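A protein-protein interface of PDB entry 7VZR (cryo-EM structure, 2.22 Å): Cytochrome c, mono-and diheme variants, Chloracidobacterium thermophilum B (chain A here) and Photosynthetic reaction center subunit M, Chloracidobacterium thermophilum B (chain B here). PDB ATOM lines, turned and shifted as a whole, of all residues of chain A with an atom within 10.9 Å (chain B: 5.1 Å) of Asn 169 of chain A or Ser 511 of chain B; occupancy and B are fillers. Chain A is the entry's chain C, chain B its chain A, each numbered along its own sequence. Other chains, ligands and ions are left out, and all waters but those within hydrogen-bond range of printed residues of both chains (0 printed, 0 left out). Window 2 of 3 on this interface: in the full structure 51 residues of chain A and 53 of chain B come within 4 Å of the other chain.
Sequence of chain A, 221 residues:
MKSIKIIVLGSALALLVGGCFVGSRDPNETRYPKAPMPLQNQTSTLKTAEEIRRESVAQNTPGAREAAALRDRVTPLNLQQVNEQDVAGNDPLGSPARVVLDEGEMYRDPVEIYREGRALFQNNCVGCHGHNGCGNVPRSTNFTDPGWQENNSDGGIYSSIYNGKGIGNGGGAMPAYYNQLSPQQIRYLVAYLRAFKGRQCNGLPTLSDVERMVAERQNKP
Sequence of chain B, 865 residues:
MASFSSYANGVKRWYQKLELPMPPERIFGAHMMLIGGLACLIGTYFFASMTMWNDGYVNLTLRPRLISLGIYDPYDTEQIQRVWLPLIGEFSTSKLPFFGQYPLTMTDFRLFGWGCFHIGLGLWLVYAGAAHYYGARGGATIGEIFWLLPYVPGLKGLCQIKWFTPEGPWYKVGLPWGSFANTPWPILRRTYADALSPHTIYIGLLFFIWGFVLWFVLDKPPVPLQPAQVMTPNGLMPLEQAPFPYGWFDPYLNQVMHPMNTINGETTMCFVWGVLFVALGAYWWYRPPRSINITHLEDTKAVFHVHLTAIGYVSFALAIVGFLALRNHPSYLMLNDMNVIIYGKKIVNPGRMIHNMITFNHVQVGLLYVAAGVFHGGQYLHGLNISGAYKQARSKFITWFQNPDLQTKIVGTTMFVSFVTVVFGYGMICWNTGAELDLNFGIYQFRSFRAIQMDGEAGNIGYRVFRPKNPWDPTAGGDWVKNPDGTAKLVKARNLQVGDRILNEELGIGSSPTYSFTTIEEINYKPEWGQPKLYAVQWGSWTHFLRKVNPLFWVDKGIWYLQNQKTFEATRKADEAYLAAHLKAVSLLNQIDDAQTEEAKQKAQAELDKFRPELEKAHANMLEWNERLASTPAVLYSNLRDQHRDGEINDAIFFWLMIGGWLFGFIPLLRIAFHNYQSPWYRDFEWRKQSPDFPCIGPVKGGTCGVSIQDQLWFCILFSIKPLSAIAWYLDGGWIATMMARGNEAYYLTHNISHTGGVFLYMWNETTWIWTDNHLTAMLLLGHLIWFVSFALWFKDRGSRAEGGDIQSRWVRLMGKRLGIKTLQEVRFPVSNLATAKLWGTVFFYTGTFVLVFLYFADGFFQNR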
ATOM      1  N   TYR A 162     -24.126   0.198  23.253  1.00  0.00           N
ATOM      2  CA  TYR A 162     -25.035   0.706  24.187  1.00  0.00           C
ATOM      3  C   TYR A 162     -25.166   2.226  24.084  1.00  0.00           C
ATOM      4  O   TYR A 162     -26.209   2.694  24.002  1.00  0.00           O
ATOM      5  CB  TYR A 162     -24.531   0.247  25.547  1.00  0.00           C
ATOM      6  CG  TYR A 162     -25.340   0.650  26.668  1.00  0.00           C
ATOM      7  CD1 TYR A 162     -25.228   1.889  27.171  1.00  0.00           C
ATOM      8  CD2 TYR A 162     -26.214  -0.211  27.221  1.00  0.00           C
ATOM      9  CE1 TYR A 162     -25.983   2.299  28.162  1.00  0.00           C
ATOM     10  CE2 TYR A 162     -26.954   0.148  28.275  1.00  0.00           C
ATOM     11  CZ  TYR A 162     -26.823   1.443  28.699  1.00  0.00           C
ATOM     12  OH  TYR A 162     -27.484   1.892  29.645  1.00  0.00           O
ATOM     13  N   ASN A 163     -24.097   2.963  23.983  1.00  0.00           N
ATOM     14  CA  ASN A 163     -24.144   4.374  23.883  1.00  0.00           C
ATOM     15  C   ASN A 163     -24.368   4.999  22.575  1.00  0.00           C
ATOM     16  O   ASN A 163     -24.890   5.956  22.527  1.00  0.00           O
ATOM     17  CB  ASN A 163     -22.848   5.023  24.390  1.00  0.00           C
ATOM     18  CG  ASN A 163     -22.636   4.839  25.833  1.00  0.00           C
ATOM     19  OD1 ASN A 163     -23.502   4.947  26.511  1.00  0.00           O
ATOM     20  ND2 ASN A 163     -21.508   4.556  26.253  1.00  0.00           N
ATOM     21  N   GLY A 164     -23.983   4.357  21.527  1.00  0.00           N
ATOM     22  CA  GLY A 164     -23.882   4.907  20.220  1.00  0.00           C
ATOM     23  C   GLY A 164     -22.512   5.602  20.111  1.00  0.00           C
ATOM     24  O   GLY A 164     -21.729   5.469  20.887  1.00  0.00           O
ATOM     25  N   LYS A 165     -22.172   6.197  19.054  1.00  0.00           N
ATOM     26  CA  LYS A 165     -20.891   6.930  18.773  1.00  0.00           C
ATOM     27  C   LYS A 165     -21.129   8.106  18.110  1.00  0.00           C
ATOM     28  O   LYS A 165     -21.751   8.056  17.190  1.00  0.00           O
ATOM     29  CB  LYS A 165     -19.850   6.017  18.340  1.00  0.00           C
ATOM     30  CG  LYS A 165     -18.531   6.559  18.531  1.00  0.00           C
ATOM     31  CD  LYS A 165     -17.530   5.495  18.431  1.00  0.00           C
ATOM     32  CE  LYS A 165     -16.304   5.988  17.810  1.00  0.00           C
ATOM     33  NZ  LYS A 165     -15.213   5.078  17.930  1.00  0.00           N
ATOM     34  N   GLY A 166     -20.692   9.213  18.623  1.00  0.00           N
ATOM     35  CA  GLY A 166     -20.868  10.530  18.034  1.00  0.00           C
ATOM     36  C   GLY A 166     -21.932  11.316  18.740  1.00  0.00           C
ATOM     37  O   GLY A 166     -22.654  10.784  19.397  1.00  0.00           O
ATOM     38  N   ILE A 167     -22.009  12.611  18.621  1.00  0.00           N
ATOM     39  CA  ILE A 167     -23.030  13.423  19.236  1.00  0.00           C
ATOM     40  C   ILE A 167     -24.366  13.429  18.428  1.00  0.00           C
ATOM     41  O   ILE A 167     -24.303  13.370  17.338  1.00  0.00           O
ATOM     42  CB  ILE A 167     -22.494  14.846  19.360  1.00  0.00           C
ATOM     43  CG1 ILE A 167     -21.240  14.932  20.240  1.00  0.00           C
ATOM     44  CG2 ILE A 167     -23.578  15.858  19.640  1.00  0.00           C
ATOM     45  CD1 ILE A 167     -20.725  16.300  20.440  1.00  0.00           C
ATOM     46  N   GLY A 168     -25.521  13.347  19.019  1.00  0.00           N
ATOM     47  CA  GLY A 168     -26.820  13.418  18.419  1.00  0.00           C
ATOM     48  C   GLY A 168     -27.886  12.891  19.347  1.00  0.00           C
ATOM     49  O   GLY A 168     -27.572  12.397  20.334  1.00  0.00           O
ATOM     50  N   ASN A 169     -29.139  13.002  19.002  1.00  0.00           N
ATOM     51  CA  ASN A 169     -30.236  12.496  19.713  1.00  0.00           C
ATOM     52  C   ASN A 169     -30.268  11.012  19.458  1.00  0.00           C
ATOM     53  O   ASN A 169     -30.230  10.673  18.339  1.00  0.00           O
ATOM     54  CB  ASN A 169     -31.516  13.069  19.156  1.00  0.00           C
ATOM     55  CG  ASN A 169     -31.693  14.543  19.389  1.00  0.00           C
ATOM     56  OD1 ASN A 169     -32.634  15.002  19.142  1.00  0.00           O
ATOM     57  ND2 ASN A 169     -30.772  15.201  19.892  1.00  0.00           N
ATOM     58  N   GLY A 170     -30.339  10.153  20.471  1.00  0.00           N
ATOM     59  CA  GLY A 170     -30.348   8.748  20.269  1.00  0.00           C
ATOM     60  C   GLY A 170     -29.032   8.171  19.818  1.00  0.00           C
ATOM     61  O   GLY A 170     -29.036   7.239  19.191  1.00  0.00           O
ATOM     62  N   GLY A 171     -27.940   8.718  20.178  1.00  0.00           N
ATOM     63  CA  GLY A 171     -26.622   8.282  19.670  1.00  0.00           C
ATOM     64  C   GLY A 171     -26.215   9.127  18.478  1.00  0.00           C
ATOM     65  O   GLY A 171     -26.926   9.961  18.144  1.00  0.00           O
ATOM     66  N   GLY A 172     -25.119   8.933  17.800  1.00  0.00           N
ATOM     67  CA  GLY A 172     -24.768   9.728  16.702  1.00  0.00           C
ATOM     68  C   GLY A 172     -24.973   9.060  15.432  1.00  0.00           C
ATOM     69  O   GLY A 172     -25.987   8.619  15.165  1.00  0.00           O
ATOM     70  N   ALA A 173     -24.005   9.102  14.562  1.00  0.00           N
ATOM     71  CA  ALA A 173     -24.140   8.393  13.321  1.00  0.00           C
ATOM     72  C   ALA A 173     -24.138   6.854  13.536  1.00  0.00           C
ATOM     73  O   ALA A 173     -24.562   6.262  12.727  1.00  0.00           O
ATOM     74  CB  ALA A 173     -23.250   8.873  12.219  1.00  0.00           C
ATOM     75  N   MET A 174     -23.479   6.329  14.564  1.00  0.00           N
ATOM     76  CA  MET A 174     -23.520   5.006  15.051  1.00  0.00           C
ATOM     77  C   MET A 174     -24.630   5.190  16.070  1.00  0.00           C
ATOM     78  O   MET A 174     -24.504   5.853  16.960  1.00  0.00           O
ATOM     79  CB  MET A 174     -22.199   4.412  15.538  1.00  0.00           C
ATOM     80  CG  MET A 174     -22.264   3.121  16.339  1.00  0.00           C
ATOM     81  SD  MET A 174     -23.495   1.866  16.114  1.00  0.00           S
ATOM     82  CE  MET A 174     -23.443   0.653  17.375  1.00  0.00           C
ATOM     83  N   PRO A 175     -25.833   4.733  15.822  1.00  0.00           N
ATOM     84  CA  PRO A 175     -26.918   4.867  16.851  1.00  0.00           C
ATOM     85  C   PRO A 175     -26.811   4.038  18.153  1.00  0.00           C
ATOM     86  O   PRO A 175     -26.189   3.153  18.189  1.00  0.00           O
ATOM     87  CB  PRO A 175     -28.184   4.497  16.073  1.00  0.00           C
ATOM     88  CG  PRO A 175     -27.718   3.823  14.870  1.00  0.00           C
ATOM     89  CD  PRO A 175     -26.285   3.973  14.651  1.00  0.00           C
ATOM     90  N   ALA A 176     -27.337   4.484  19.245  1.00  0.00           N
ATOM     91  CA  ALA A 176     -27.372   3.842  20.505  1.00  0.00           C
ATOM     92  C   ALA A 176     -28.395   2.736  20.477  1.00  0.00           C
ATOM     93  O   ALA A 176     -29.233   2.780  19.837  1.00  0.00           O
ATOM     94  CB  ALA A 176     -27.650   4.856  21.603  1.00  0.00           C
ATOM     95  N   TYR A 177     -28.236   1.707  21.225  1.00  0.00           N
ATOM     96  CA  TYR A 177     -29.113   0.610  21.323  1.00  0.00           C
ATOM     97  C   TYR A 177     -29.697   0.401  22.740  1.00  0.00           C
ATOM     98  O   TYR A 177     -30.390  -0.451  22.835  1.00  0.00           O
ATOM     99  CB  TYR A 177     -28.456  -0.684  20.714  1.00  0.00           C
ATOM    100  CG  TYR A 177     -28.465  -0.630  19.240  1.00  0.00           C
ATOM    101  CD1 TYR A 177     -27.447  -0.020  18.575  1.00  0.00           C
ATOM    102  CD2 TYR A 177     -29.522  -1.138  18.486  1.00  0.00           C
ATOM    103  CE1 TYR A 177     -27.528   0.252  17.307  1.00  0.00           C
ATOM    104  CE2 TYR A 177     -29.562  -0.983  17.150  1.00  0.00           C
ATOM    105  CZ  TYR A 177     -28.514  -0.309  16.560  1.00  0.00           C
ATOM    106  OH  TYR A 177     -28.402  -0.055  15.316  1.00  0.00           O
ATOM    107  N   TYR A 178     -29.439   1.172  23.821  1.00  0.00           N
ATOM    108  CA  TYR A 178     -29.967   0.903  25.161  1.00  0.00           C
ATOM    109  C   TYR A 178     -31.482   0.726  25.439  1.00  0.00           C
ATOM    110  O   TYR A 178     -31.802   0.092  26.222  1.00  0.00           O
ATOM    111  CB  TYR A 178     -29.277   1.789  26.132  1.00  0.00           C
ATOM    112  CG  TYR A 178     -29.758   3.156  26.039  1.00  0.00           C
ATOM    113  CD1 TYR A 178     -30.991   3.396  26.481  1.00  0.00           C
ATOM    114  CD2 TYR A 178     -29.031   4.151  25.440  1.00  0.00           C
ATOM    115  CE1 TYR A 178     -31.535   4.563  26.368  1.00  0.00           C
ATOM    116  CE2 TYR A 178     -29.527   5.415  25.341  1.00  0.00           C
ATOM    117  CZ  TYR A 178     -30.821   5.555  25.827  1.00  0.00           C
ATOM    118  OH  TYR A 178     -31.481   6.605  25.932  1.00  0.00           O
ATOM    119  N   GLN A 180     -34.204  -0.641  22.479  1.00  0.00           N
ATOM    120  CA  GLN A 180     -33.788  -1.687  21.471  1.00  0.00           C
ATOM    121  C   GLN A 180     -33.186  -3.097  21.797  1.00  0.00           C
ATOM    122  O   GLN A 180     -33.824  -3.974  21.684  1.00  0.00           O
ATOM    123  CB  GLN A 180     -33.130  -1.092  20.211  1.00  0.00           C
ATOM    124  CG  GLN A 180     -33.699  -1.516  18.895  1.00  0.00           C
ATOM    125  CD  GLN A 180     -33.251  -0.754  17.666  1.00  0.00           C
ATOM    126  OE1 GLN A 180     -33.094  -1.290  16.669  1.00  0.00           O
ATOM    127  NE2 GLN A 180     -33.043   0.440  17.764  1.00  0.00           N
ATOM    128  N   GLU B 436     -38.313  18.330  21.176  1.00  0.00           N
ATOM    129  CA  GLU B 436     -37.305  17.298  21.093  1.00  0.00           C
ATOM    130  C   GLU B 436     -36.058  17.760  20.353  1.00  0.00           C
ATOM    131  O   GLU B 436     -34.999  17.211  20.565  1.00  0.00           O
ATOM    132  CB  GLU B 436     -37.898  16.034  20.484  1.00  0.00           C
ATOM    133  CG  GLU B 436     -37.836  15.861  18.998  1.00  0.00           C
ATOM    134  CD  GLU B 436     -38.824  14.891  18.509  1.00  0.00           C
ATOM    135  OE1 GLU B 436     -39.317  15.024  17.401  1.00  0.00           O
ATOM    136  OE2 GLU B 436     -39.184  14.015  19.302  1.00  0.00           O
ATOM    137  N   LEU B 437     -36.135  18.762  19.500  1.00  0.00           N
ATOM    138  CA  LEU B 437     -34.926  19.199  18.810  1.00  0.00           C
ATOM    139  C   LEU B 437     -34.196  20.361  19.465  1.00  0.00           C
ATOM    140  O   LEU B 437     -33.187  20.729  18.939  1.00  0.00           O
ATOM    141  CB  LEU B 437     -35.234  19.604  17.384  1.00  0.00           C
ATOM    142  CG  LEU B 437     -35.558  18.577  16.283  1.00  0.00           C
ATOM    143  CD1 LEU B 437     -35.893  19.233  14.964  1.00  0.00           C
ATOM    144  CD2 LEU B 437     -34.514  17.565  16.103  1.00  0.00           C
ATOM    145  N   ASP B 438     -34.763  21.014  20.482  1.00  0.00           N
ATOM    146  CA  ASP B 438     -34.189  22.123  21.283  1.00  0.00           C
ATOM    147  C   ASP B 438     -34.008  23.398  20.499  1.00  0.00           C
ATOM    148  O   ASP B 438     -33.011  24.057  20.652  1.00  0.00           O
ATOM    149  CB  ASP B 438     -32.860  21.762  21.916  1.00  0.00           C
ATOM    150  CG  ASP B 438     -32.967  20.859  23.087  1.00  0.00           C
ATOM    151  OD1 ASP B 438     -33.492  21.249  24.081  1.00  0.00           O
ATOM    152  OD2 ASP B 438     -32.445  19.808  22.993  1.00  0.00           O
ATOM    153  N   ILE B 509     -24.104  16.178  27.132  1.00  0.00           N
ATOM    154  CA  ILE B 509     -25.095  16.451  26.102  1.00  0.00           C
ATOM    155  C   ILE B 509     -24.503  17.472  25.136  1.00  0.00           C
ATOM    156  O   ILE B 509     -24.193  18.589  25.535  1.00  0.00           O
ATOM    157  CB  ILE B 509     -26.410  16.967  26.725  1.00  0.00           C
ATOM    158  CG1 ILE B 509     -27.007  15.991  27.707  1.00  0.00           C
ATOM    159  CG2 ILE B 509     -27.447  17.472  25.717  1.00  0.00           C
ATOM    160  CD1 ILE B 509     -27.798  16.654  28.638  1.00  0.00           C
ATOM    161  N   GLY B 510     -24.255  17.068  23.915  1.00  0.00           N
ATOM    162  CA  GLY B 510     -24.190  17.953  22.802  1.00  0.00           C
ATOM    163  C   GLY B 510     -25.581  18.107  22.270  1.00  0.00           C
ATOM    164  O   GLY B 510     -26.569  17.841  22.942  1.00  0.00           O
ATOM    165  N   SER B 511     -25.687  18.449  21.053  1.00  0.00           N
ATOM    166  CA  SER B 511     -27.032  18.413  20.477  1.00  0.00           C
ATOM    167  C   SER B 511     -27.989  19.438  21.046  1.00  0.00           C
ATOM    168  O   SER B 511     -29.059  19.602  20.491  1.00  0.00           O
ATOM    169  CB  SER B 511     -27.609  16.992  20.531  1.00  0.00           C
ATOM    170  OG  SER B 511     -28.322  16.713  21.689  1.00  0.00           O
ATOM    171  N   SER B 512     -27.668  20.174  22.077  1.00  0.00           N
ATOM    172  CA  SER B 512     -28.437  21.366  22.410  1.00  0.00           C
ATOM    173  C   SER B 512     -27.547  22.580  22.570  1.00  0.00           C
ATOM    174  O   SER B 512     -27.684  23.284  23.546  1.00  0.00           O
ATOM    175  CB  SER B 512     -29.342  21.180  23.629  1.00  0.00           C
ATOM    176  OG  SER B 512     -28.782  21.506  24.839  1.00  0.00           O
ATOM    177  N   PRO B 513     -26.860  22.997  21.502  1.00  0.00           N
ATOM    178  CA  PRO B 513     -25.839  24.037  21.616  1.00  0.00           C
ATOM    179  C   PRO B 513     -26.330  25.470  21.917  1.00  0.00           C
ATOM    180  O   PRO B 513     -25.525  26.299  22.229  1.00  0.00           O
ATOM    181  CB  PRO B 513     -25.174  23.958  20.250  1.00  0.00           C
ATOM    182  CG  PRO B 513     -26.073  23.445  19.468  1.00  0.00           C
ATOM    183  CD  PRO B 513     -26.844  22.477  20.140  1.00  0.00           C
ATOM    184  N   ARG B 742     -36.378   9.496  18.410  1.00  0.00           N
ATOM    185  CA  ARG B 742     -35.606   8.244  18.292  1.00  0.00           C
ATOM    186  C   ARG B 742     -36.064   7.252  19.341  1.00  0.00           C
ATOM    187  O   ARG B 742     -36.531   7.626  20.266  1.00  0.00           O
ATOM    188  CB  ARG B 742     -34.073   8.426  18.371  1.00  0.00           C
ATOM    189  CG  ARG B 742     -33.428   8.843  17.077  1.00  0.00           C
ATOM    190  CD  ARG B 742     -33.554  10.260  17.032  1.00  0.00           C
ATOM    191  NE  ARG B 742     -32.494  10.810  16.250  1.00  0.00           N
ATOM    192  CZ  ARG B 742     -32.376  12.043  15.830  1.00  0.00           C
ATOM    193  NH1 ARG B 742     -31.340  12.382  15.270  1.00  0.00           N
ATOM    194  NH2 ARG B 742     -33.325  12.873  15.865  1.00  0.00           N
ATOM    195  N   GLU B 745     -34.035   7.040  23.670  1.00  0.00           N
ATOM    196  CA  GLU B 745     -33.800   8.256  24.409  1.00  0.00           C
ATOM    197  C   GLU B 745     -34.547   8.214  25.719  1.00  0.00           C
ATOM    198  O   GLU B 745     -35.338   7.325  25.946  1.00  0.00           O
ATOM    199  CB  GLU B 745     -34.078   9.508  23.628  1.00  0.00           C
ATOM    200  CG  GLU B 745     -35.110   9.538  22.839  1.00  0.00           C
ATOM    201  CD  GLU B 745     -34.849  10.486  21.731  1.00  0.00           C
ATOM    202  OE1 GLU B 745     -35.731  11.155  21.186  1.00  0.00           O
ATOM    203  OE2 GLU B 745     -33.690  10.594  21.404  1.00  0.00           O
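The side-chain carboxylate (OE1) of Glu 745 of chain B is in hydrogen-bond range of the backbone NH (N) of Arg 742 of chain B.
O of Gly 170 of chain A lies within hydrogen-bond range of N of Ala 176 of chain A (3.2 Å).
OH of Tyr 178 of chain A sits close to N of Glu 745 of chain B (3.4 Å).
The side-chain hydroxyl (OG) of Ser 511 of chain B sits at hydrogen-bond distance from the side-chain amide nitrogen (ND2) of Asn 169 of chain A (3.4 Å).
The guanidinium group of Arg 742 of chain B is in hydrogen-bond range of the backbone carbonyl oxygen of Asn 169 of chain A (3.1 Å).
Printed residues of chain A that touch a printed residue of chain B: Ile 167, Asn 169, Gly 170 and Tyr 178.
Hydrophobic or aromatic side chains of chain A that line the printed part of chain B: Ile 167 and Tyr 178.
Among the printed residues, no Asp or Glu carboxylate lies within 4 Å of a Lys or Arg side-chain nitrogen of the other chain.
Among the printed residues, pairs that only touch across the chains: Gly 170 of chain A with Glu 745 of chain B, Asn 169 of chain A with Glu 436 of chain B, Ile 167 of chain A with Ser 511 of chain B, Ile 167 of chain A with Gly 510 of chain B and Asn 169 of chain A with Glu 745 of chain B.
Asn 169 of chain A touches just these residues of chain B: Glu 436, Ser 511, Arg 742 and Glu 745.
Of chain A, only Ile 167 (3.6 Å) and Asn 169 (3.4 Å) come within 4 Å of Ser 511 of chain B.
No residue of chain A comes within 4 Å of Leu 437 of chain B.
No residue of chain A comes within 4 Å of Asp 438 of chain B.
Of chain A, only Ile 167 comes within 4 Å of Gly 510 of chain B.
No residue of chain A comes within 4 Å of Ser 512 of chain B.
Printed residues of chain B within 4 Å of Ile 167 of chain A: Gly 510 and Ser 511.
Of the printed residues of chain B, Tyr 178 of chain A touches Glu 745.
Met 174 of chain A touches none of the printed residues of chain B.
The nearest residue of chain B that does not touch Asn 169 of chain A is Leu 437 of chain B (4.4 Å).
The nearest residue of chain A that does not touch Ser 511 of chain B is Gly 168 of chain A (4.2 Å).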
